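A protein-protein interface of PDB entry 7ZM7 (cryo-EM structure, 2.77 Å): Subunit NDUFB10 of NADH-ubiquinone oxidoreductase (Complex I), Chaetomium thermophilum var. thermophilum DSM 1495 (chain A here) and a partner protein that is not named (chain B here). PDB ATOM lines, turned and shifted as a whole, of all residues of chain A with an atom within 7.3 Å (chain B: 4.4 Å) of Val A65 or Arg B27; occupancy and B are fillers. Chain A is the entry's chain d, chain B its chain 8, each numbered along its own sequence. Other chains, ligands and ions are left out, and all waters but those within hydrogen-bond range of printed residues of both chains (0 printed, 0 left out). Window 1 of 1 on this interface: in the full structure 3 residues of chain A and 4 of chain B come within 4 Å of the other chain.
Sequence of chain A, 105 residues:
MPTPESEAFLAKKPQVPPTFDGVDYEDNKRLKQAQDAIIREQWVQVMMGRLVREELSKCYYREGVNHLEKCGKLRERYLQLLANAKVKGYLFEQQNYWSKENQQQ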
ATOM      1  N   TYR A  60     -18.342  10.212 -25.945  1.00  0.00           N
ATOM      2  CA  TYR A  60     -18.633  11.141 -27.031  1.00  0.00           C
ATOM      3  C   TYR A  60     -20.055  11.670 -26.939  1.00  0.00           C
ATOM      4  O   TYR A  60     -20.280  12.880 -27.002  1.00  0.00           O
ATOM      5  CB  TYR A  60     -18.414  10.452 -28.374  1.00  0.00           C
ATOM      6  CG  TYR A  60     -18.671  11.335 -29.570  1.00  0.00           C
ATOM      7  CD1 TYR A  60     -19.936  11.428 -30.134  1.00  0.00           C
ATOM      8  CD2 TYR A  60     -17.652  12.068 -30.130  1.00  0.00           C
ATOM      9  CE1 TYR A  60     -20.171  12.236 -31.210  1.00  0.00           C
ATOM     10  CE2 TYR A  60     -17.877  12.859 -31.213  1.00  0.00           C
ATOM     11  CZ  TYR A  60     -19.135  12.949 -31.746  1.00  0.00           C
ATOM     12  OH  TYR A  60     -19.339  13.754 -32.826  1.00  0.00           O
ATOM     13  N   TYR A  61     -21.028  10.779 -26.793  1.00  0.00           N
ATOM     14  CA  TYR A  61     -22.419  11.200 -26.714  1.00  0.00           C
ATOM     15  C   TYR A  61     -22.763  11.845 -25.387  1.00  0.00           C
ATOM     16  O   TYR A  61     -23.724  12.614 -25.323  1.00  0.00           O
ATOM     17  CB  TYR A  61     -23.343  10.015 -26.976  1.00  0.00           C
ATOM     18  CG  TYR A  61     -23.315   9.642 -28.423  1.00  0.00           C
ATOM     19  CD1 TYR A  61     -23.633  10.570 -29.391  1.00  0.00           C
ATOM     20  CD2 TYR A  61     -22.918   8.394 -28.827  1.00  0.00           C
ATOM     21  CE1 TYR A  61     -23.580  10.253 -30.712  1.00  0.00           C
ATOM     22  CE2 TYR A  61     -22.856   8.073 -30.147  1.00  0.00           C
ATOM     23  CZ  TYR A  61     -23.190   9.001 -31.083  1.00  0.00           C
ATOM     24  OH  TYR A  61     -23.137   8.676 -32.417  1.00  0.00           O
ATOM     25  N   ARG A  62     -22.005  11.550 -24.336  1.00  0.00           N
ATOM     26  CA  ARG A  62     -22.220  12.205 -23.057  1.00  0.00           C
ATOM     27  C   ARG A  62     -21.777  13.659 -23.092  1.00  0.00           C
ATOM     28  O   ARG A  62     -22.444  14.528 -22.523  1.00  0.00           O
ATOM     29  CB  ARG A  62     -21.507  11.429 -21.953  1.00  0.00           C
ATOM     30  CG  ARG A  62     -21.744  11.947 -20.568  1.00  0.00           C
ATOM     31  CD  ARG A  62     -21.076  11.086 -19.519  1.00  0.00           C
ATOM     32  NE  ARG A  62     -19.620  11.068 -19.612  1.00  0.00           N
ATOM     33  CZ  ARG A  62     -18.911   9.986 -19.930  1.00  0.00           C
ATOM     34  NH1 ARG A  62     -17.590  10.055 -19.997  1.00  0.00           N
ATOM     35  NH2 ARG A  62     -19.516   8.827 -20.141  1.00  0.00           N
ATOM     36  N   GLU A  63     -20.694  13.959 -23.790  1.00  0.00           N
ATOM     37  CA  GLU A  63     -20.123  15.291 -23.690  1.00  0.00           C
ATOM     38  C   GLU A  63     -20.473  16.187 -24.863  1.00  0.00           C
ATOM     39  O   GLU A  63     -20.504  17.409 -24.706  1.00  0.00           O
ATOM     40  CB  GLU A  63     -18.607  15.201 -23.537  1.00  0.00           C
ATOM     41  CG  GLU A  63     -18.146  14.106 -22.602  1.00  0.00           C
ATOM     42  CD  GLU A  63     -18.554  14.321 -21.168  1.00  0.00           C
ATOM     43  OE1 GLU A  63     -19.008  15.431 -20.825  1.00  0.00           O
ATOM     44  OE2 GLU A  63     -18.410  13.372 -20.370  1.00  0.00           O
ATOM     45  N   GLY A  64     -20.726  15.616 -26.034  1.00  0.00           N
ATOM     46  CA  GLY A  64     -21.274  16.378 -27.130  1.00  0.00           C
ATOM     47  C   GLY A  64     -20.291  17.341 -27.747  1.00  0.00           C
ATOM     48  O   GLY A  64     -19.385  16.916 -28.462  1.00  0.00           O
ATOM     49  N   VAL A  65     -20.471  18.640 -27.513  1.00  0.00           N
ATOM     50  CA  VAL A  65     -19.494  19.599 -28.012  1.00  0.00           C
ATOM     51  C   VAL A  65     -18.177  19.457 -27.258  1.00  0.00           C
ATOM     52  O   VAL A  65     -17.093  19.572 -27.842  1.00  0.00           O
ATOM     53  CB  VAL A  65     -20.045  21.033 -27.936  1.00  0.00           C
ATOM     54  CG1 VAL A  65     -20.313  21.444 -26.514  1.00  0.00           C
ATOM     55  CG2 VAL A  65     -19.087  21.985 -28.589  1.00  0.00           C
ATOM     56  N   ASN A  66     -18.248  19.169 -25.960  1.00  0.00           N
ATOM     57  CA  ASN A  66     -17.078  19.053 -25.108  1.00  0.00           C
ATOM     58  C   ASN A  66     -16.380  17.712 -25.238  1.00  0.00           C
ATOM     59  O   ASN A  66     -15.537  17.399 -24.401  1.00  0.00           O
ATOM     60  CB  ASN A  66     -17.470  19.295 -23.650  1.00  0.00           C
ATOM     61  CG  ASN A  66     -18.063  20.672 -23.423  1.00  0.00           C
ATOM     62  OD1 ASN A  66     -17.430  21.683 -23.693  1.00  0.00           O
ATOM     63  ND2 ASN A  66     -19.290  20.713 -22.943  1.00  0.00           N
ATOM     64  N   HIS A  67     -16.697  16.899 -26.245  1.00  0.00           N
ATOM     65  CA  HIS A  67     -15.960  15.652 -26.423  1.00  0.00           C
ATOM     66  C   HIS A  67     -14.484  15.895 -26.699  1.00  0.00           C
ATOM     67  O   HIS A  67     -13.656  15.058 -26.341  1.00  0.00           O
ATOM     68  CB  HIS A  67     -16.563  14.816 -27.552  1.00  0.00           C
ATOM     69  CG  HIS A  67     -16.068  15.188 -28.910  1.00  0.00           C
ATOM     70  ND1 HIS A  67     -15.053  14.509 -29.544  1.00  0.00           N
ATOM     71  CD2 HIS A  67     -16.437  16.180 -29.748  1.00  0.00           C
ATOM     72  CE1 HIS A  67     -14.819  15.067 -30.717  1.00  0.00           C
ATOM     73  NE2 HIS A  67     -15.650  16.079 -30.867  1.00  0.00           N
ATOM     74  N   LEU A  68     -14.136  17.035 -27.270  1.00  0.00           N
ATOM     75  CA  LEU A  68     -12.775  17.332 -27.680  1.00  0.00           C
ATOM     76  C   LEU A  68     -11.834  17.567 -26.510  1.00  0.00           C
ATOM     77  O   LEU A  68     -10.633  17.732 -26.725  1.00  0.00           O
ATOM     78  CB  LEU A  68     -12.765  18.546 -28.610  1.00  0.00           C
ATOM     79  CG  LEU A  68     -12.850  18.214 -30.092  1.00  0.00           C
ATOM     80  CD1 LEU A  68     -13.219  19.404 -30.933  1.00  0.00           C
ATOM     81  CD2 LEU A  68     -11.521  17.702 -30.502  1.00  0.00           C
ATOM     82  N   GLU A  69     -12.348  17.588 -25.287  1.00  0.00           N
ATOM     83  CA  GLU A  69     -11.527  17.792 -24.110  1.00  0.00           C
ATOM     84  C   GLU A  69     -11.693  16.727 -23.051  1.00  0.00           C
ATOM     85  O   GLU A  69     -10.791  16.570 -22.226  1.00  0.00           O
ATOM     86  CB  GLU A  69     -11.842  19.149 -23.481  1.00  0.00           C
ATOM     87  CG  GLU A  69     -13.299  19.324 -23.129  1.00  0.00           C
ATOM     88  CD  GLU A  69     -13.635  18.785 -21.752  1.00  0.00           C
ATOM     89  OE1 GLU A  69     -12.713  18.669 -20.916  1.00  0.00           O
ATOM     90  OE2 GLU A  69     -14.819  18.470 -21.511  1.00  0.00           O
ATOM     91  N   MET B  17     -17.378  28.667 -19.254  1.00  0.00           N
ATOM     92  CA  MET B  17     -18.002  28.582 -20.597  1.00  0.00           C
ATOM     93  C   MET B  17     -18.272  27.132 -20.986  1.00  0.00           C
ATOM     94  O   MET B  17     -19.293  26.900 -21.659  1.00  0.00           O
ATOM     95  CB  MET B  17     -17.106  29.215 -21.660  1.00  0.00           C
ATOM     96  CG  MET B  17     -17.271  30.710 -21.742  1.00  0.00           C
ATOM     97  SD  MET B  17     -16.323  31.422 -23.094  1.00  0.00           S
ATOM     98  CE  MET B  17     -16.765  33.147 -22.904  1.00  0.00           C
ATOM     99  N   ARG B  18     -17.412  26.190 -20.582  1.00  0.00           N
ATOM    100  CA  ARG B  18     -17.671  24.843 -21.068  1.00  0.00           C
ATOM    101  C   ARG B  18     -18.813  24.178 -20.321  1.00  0.00           C
ATOM    102  O   ARG B  18     -19.452  23.270 -20.859  1.00  0.00           O
ATOM    103  CB  ARG B  18     -16.409  23.990 -20.951  1.00  0.00           C
ATOM    104  CG  ARG B  18     -16.250  23.311 -19.608  1.00  0.00           C
ATOM    105  CD  ARG B  18     -15.306  22.149 -19.677  1.00  0.00           C
ATOM    106  NE  ARG B  18     -14.995  21.631 -18.348  1.00  0.00           N
ATOM    107  CZ  ARG B  18     -13.876  21.891 -17.681  1.00  0.00           C
ATOM    108  NH1 ARG B  18     -13.687  21.374 -16.475  1.00  0.00           N
ATOM    109  NH2 ARG B  18     -12.944  22.667 -18.217  1.00  0.00           N
ATOM    110  N   LYS B  21     -22.022  24.537 -22.092  1.00  0.00           N
ATOM    111  CA  LYS B  21     -22.020  23.942 -23.426  1.00  0.00           C
ATOM    112  C   LYS B  21     -22.313  24.980 -24.503  1.00  0.00           C
ATOM    113  O   LYS B  21     -23.059  24.727 -25.451  1.00  0.00           O
ATOM    114  CB  LYS B  21     -23.014  22.786 -23.509  1.00  0.00           C
ATOM    115  CG  LYS B  21     -22.624  21.582 -22.687  1.00  0.00           C
ATOM    116  CD  LYS B  21     -23.683  20.512 -22.767  1.00  0.00           C
ATOM    117  CE  LYS B  21     -23.678  19.900 -24.152  1.00  0.00           C
ATOM    118  NZ  LYS B  21     -22.422  19.138 -24.366  1.00  0.00           N
ATOM    119  N   VAL B  22     -21.735  26.161 -24.346  1.00  0.00           N
ATOM    120  CA  VAL B  22     -21.794  27.179 -25.398  1.00  0.00           C
ATOM    121  C   VAL B  22     -21.039  26.675 -26.623  1.00  0.00           C
ATOM    122  O   VAL B  22     -20.031  25.968 -26.474  1.00  0.00           O
ATOM    123  CB  VAL B  22     -21.225  28.500 -24.874  1.00  0.00           C
ATOM    124  CG1 VAL B  22     -19.770  28.369 -24.548  1.00  0.00           C
ATOM    125  CG2 VAL B  22     -21.429  29.620 -25.867  1.00  0.00           C
ATOM    126  N   PRO B  23     -21.521  26.935 -27.838  1.00  0.00           N
ATOM    127  CA  PRO B  23     -20.865  26.377 -29.023  1.00  0.00           C
ATOM    128  C   PRO B  23     -19.460  26.920 -29.195  1.00  0.00           C
ATOM    129  O   PRO B  23     -19.155  28.053 -28.824  1.00  0.00           O
ATOM    130  CB  PRO B  23     -21.781  26.813 -30.167  1.00  0.00           C
ATOM    131  CG  PRO B  23     -23.095  27.003 -29.532  1.00  0.00           C
ATOM    132  CD  PRO B  23     -22.820  27.536 -28.177  1.00  0.00           C
ATOM    133  N   LEU B  24     -18.604  26.092 -29.790  1.00  0.00           N
ATOM    134  CA  LEU B  24     -17.165  26.286 -29.651  1.00  0.00           C
ATOM    135  C   LEU B  24     -16.704  27.612 -30.232  1.00  0.00           C
ATOM    136  O   LEU B  24     -15.993  28.370 -29.570  1.00  0.00           O
ATOM    137  CB  LEU B  24     -16.416  25.128 -30.297  1.00  0.00           C
ATOM    138  CG  LEU B  24     -16.239  23.977 -29.323  1.00  0.00           C
ATOM    139  CD1 LEU B  24     -15.455  22.838 -29.942  1.00  0.00           C
ATOM    140  CD2 LEU B  24     -15.552  24.489 -28.104  1.00  0.00           C
ATOM    141  N   ALA B  25     -17.100  27.912 -31.468  1.00  0.00           N
ATOM    142  CA  ALA B  25     -16.592  29.110 -32.125  1.00  0.00           C
ATOM    143  C   ALA B  25     -17.113  30.383 -31.481  1.00  0.00           C
ATOM    144  O   ALA B  25     -16.627  31.467 -31.804  1.00  0.00           O
ATOM    145  CB  ALA B  25     -16.947  29.089 -33.608  1.00  0.00           C
ATOM    146  N   TYR B  26     -18.089  30.275 -30.586  1.00  0.00           N
ATOM    147  CA  TYR B  26     -18.664  31.426 -29.909  1.00  0.00           C
ATOM    148  C   TYR B  26     -18.182  31.554 -28.481  1.00  0.00           C
ATOM    149  O   TYR B  26     -18.831  32.221 -27.680  1.00  0.00           O
ATOM    150  CB  TYR B  26     -20.184  31.340 -29.936  1.00  0.00           C
ATOM    151  CG  TYR B  26     -20.751  31.415 -31.324  1.00  0.00           C
ATOM    152  CD1 TYR B  26     -20.105  32.134 -32.316  1.00  0.00           C
ATOM    153  CD2 TYR B  26     -21.918  30.749 -31.652  1.00  0.00           C
ATOM    154  CE1 TYR B  26     -20.613  32.199 -33.589  1.00  0.00           C
ATOM    155  CE2 TYR B  26     -22.435  30.808 -32.925  1.00  0.00           C
ATOM    156  CZ  TYR B  26     -21.780  31.534 -33.888  1.00  0.00           C
ATOM    157  OH  TYR B  26     -22.294  31.593 -35.160  1.00  0.00           O
ATOM    158  N   ARG B  27     -17.066  30.931 -28.136  1.00  0.00           N
ATOM    159  CA  ARG B  27     -16.513  31.073 -26.793  1.00  0.00           C
ATOM    160  C   ARG B  27     -15.571  32.256 -26.727  1.00  0.00           C
ATOM    161  O   ARG B  27     -14.508  32.215 -26.123  1.00  0.00           O
ATOM    162  CB  ARG B  27     -15.818  29.788 -26.381  1.00  0.00           C
ATOM    163  CG  ARG B  27     -16.792  28.671 -26.168  1.00  0.00           C
ATOM    164  CD  ARG B  27     -16.139  27.422 -25.721  1.00  0.00           C
ATOM    165  NE  ARG B  27     -17.060  26.309 -25.846  1.00  0.00           N
ATOM    166  CZ  ARG B  27     -17.079  25.269 -25.028  1.00  0.00           C
ATOM    167  NH1 ARG B  27     -16.220  25.198 -24.024  1.00  0.00           N
ATOM    168  NH2 ARG B  27     -17.955  24.300 -25.215  1.00  0.00           N
ATOM    169  N   ASP B  28     -16.012  33.347 -27.330  1.00  0.00           N
ATOM    170  CA  ASP B  28     -15.203  34.534 -27.510  1.00  0.00           C
ATOM    171  C   ASP B  28     -15.364  35.458 -26.308  1.00  0.00           C
ATOM    172  O   ASP B  28     -15.950  35.094 -25.286  1.00  0.00           O
ATOM    173  CB  ASP B  28     -15.572  35.207 -28.831  1.00  0.00           C
ATOM    174  CG  ASP B  28     -17.016  35.680 -28.863  1.00  0.00           C
ATOM    175  OD1 ASP B  28     -17.746  35.450 -27.877  1.00  0.00           O
ATOM    176  OD2 ASP B  28     -17.425  36.286 -29.878  1.00  0.00           O
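The backbone carbonyl oxygen (O) of Arg B18 lies within hydrogen-bond range of the side-chain amide nitrogen (ND2) of Asn A66. The side-chain amide oxygen (OD1) of Asn A66 lies within hydrogen-bond range of the guanidinium group (NH2) of Arg B27 (3.1 Å). The side-chain amino group (NZ) of Lys B21 sits at hydrogen-bond distance from the backbone carbonyl oxygen (O) of Glu A63 (2.6 Å).
O of Val B22 is in hydrogen-bond range of NH2 of Arg B27, 2.9 Å away. OE2 of Glu A63 lies within salt-bridge range of NE of Arg A62.
Among the printed residues, merely in contact across the chains: Val A65 with Lys B21, Val A65 with Leu B24, Val A65 with Arg B27 and Asn A66 with Lys B21.
Printed residues of chain B within 4 Å of Glu A63: Lys B21 (2.6 Å). Of the printed residues of chain B, Asn A66 touches Arg B18 (3.3 Å), Lys B21 (3.5 Å) and Arg B27 (3.1 Å). Printed residues of chain A within 4 Å of Arg B18: Asn A66. Of the printed residues of chain A, Lys B21 touches Glu A63, Val A65 and Asn A66. Of the printed residues of chain A, Leu B24 touches Val A65. The nearest residue of chain A that does not touch Arg B27 is Glu A69 (6.6 Å). The nearest printed residue of chain A that does not touch Arg B18 is Glu A69 (4.1 Å).
Printed residues of chain A that touch a printed residue of chain B: Glu A63, Val A65 and Asn A66. Hydrophobic or aromatic side chains of chain A that line the printed part of chain B: Val A65. Of the 10 printed residues of chain B, 4 touch a printed residue of chain A. Hydrophobic or aromatic side chains of chain B that line the printed part of chain A: Leu B24. Among the printed residues, no Asp or Glu carboxylate lies within 4 Å of a Lys or Arg side-chain nitrogen of the other chain.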
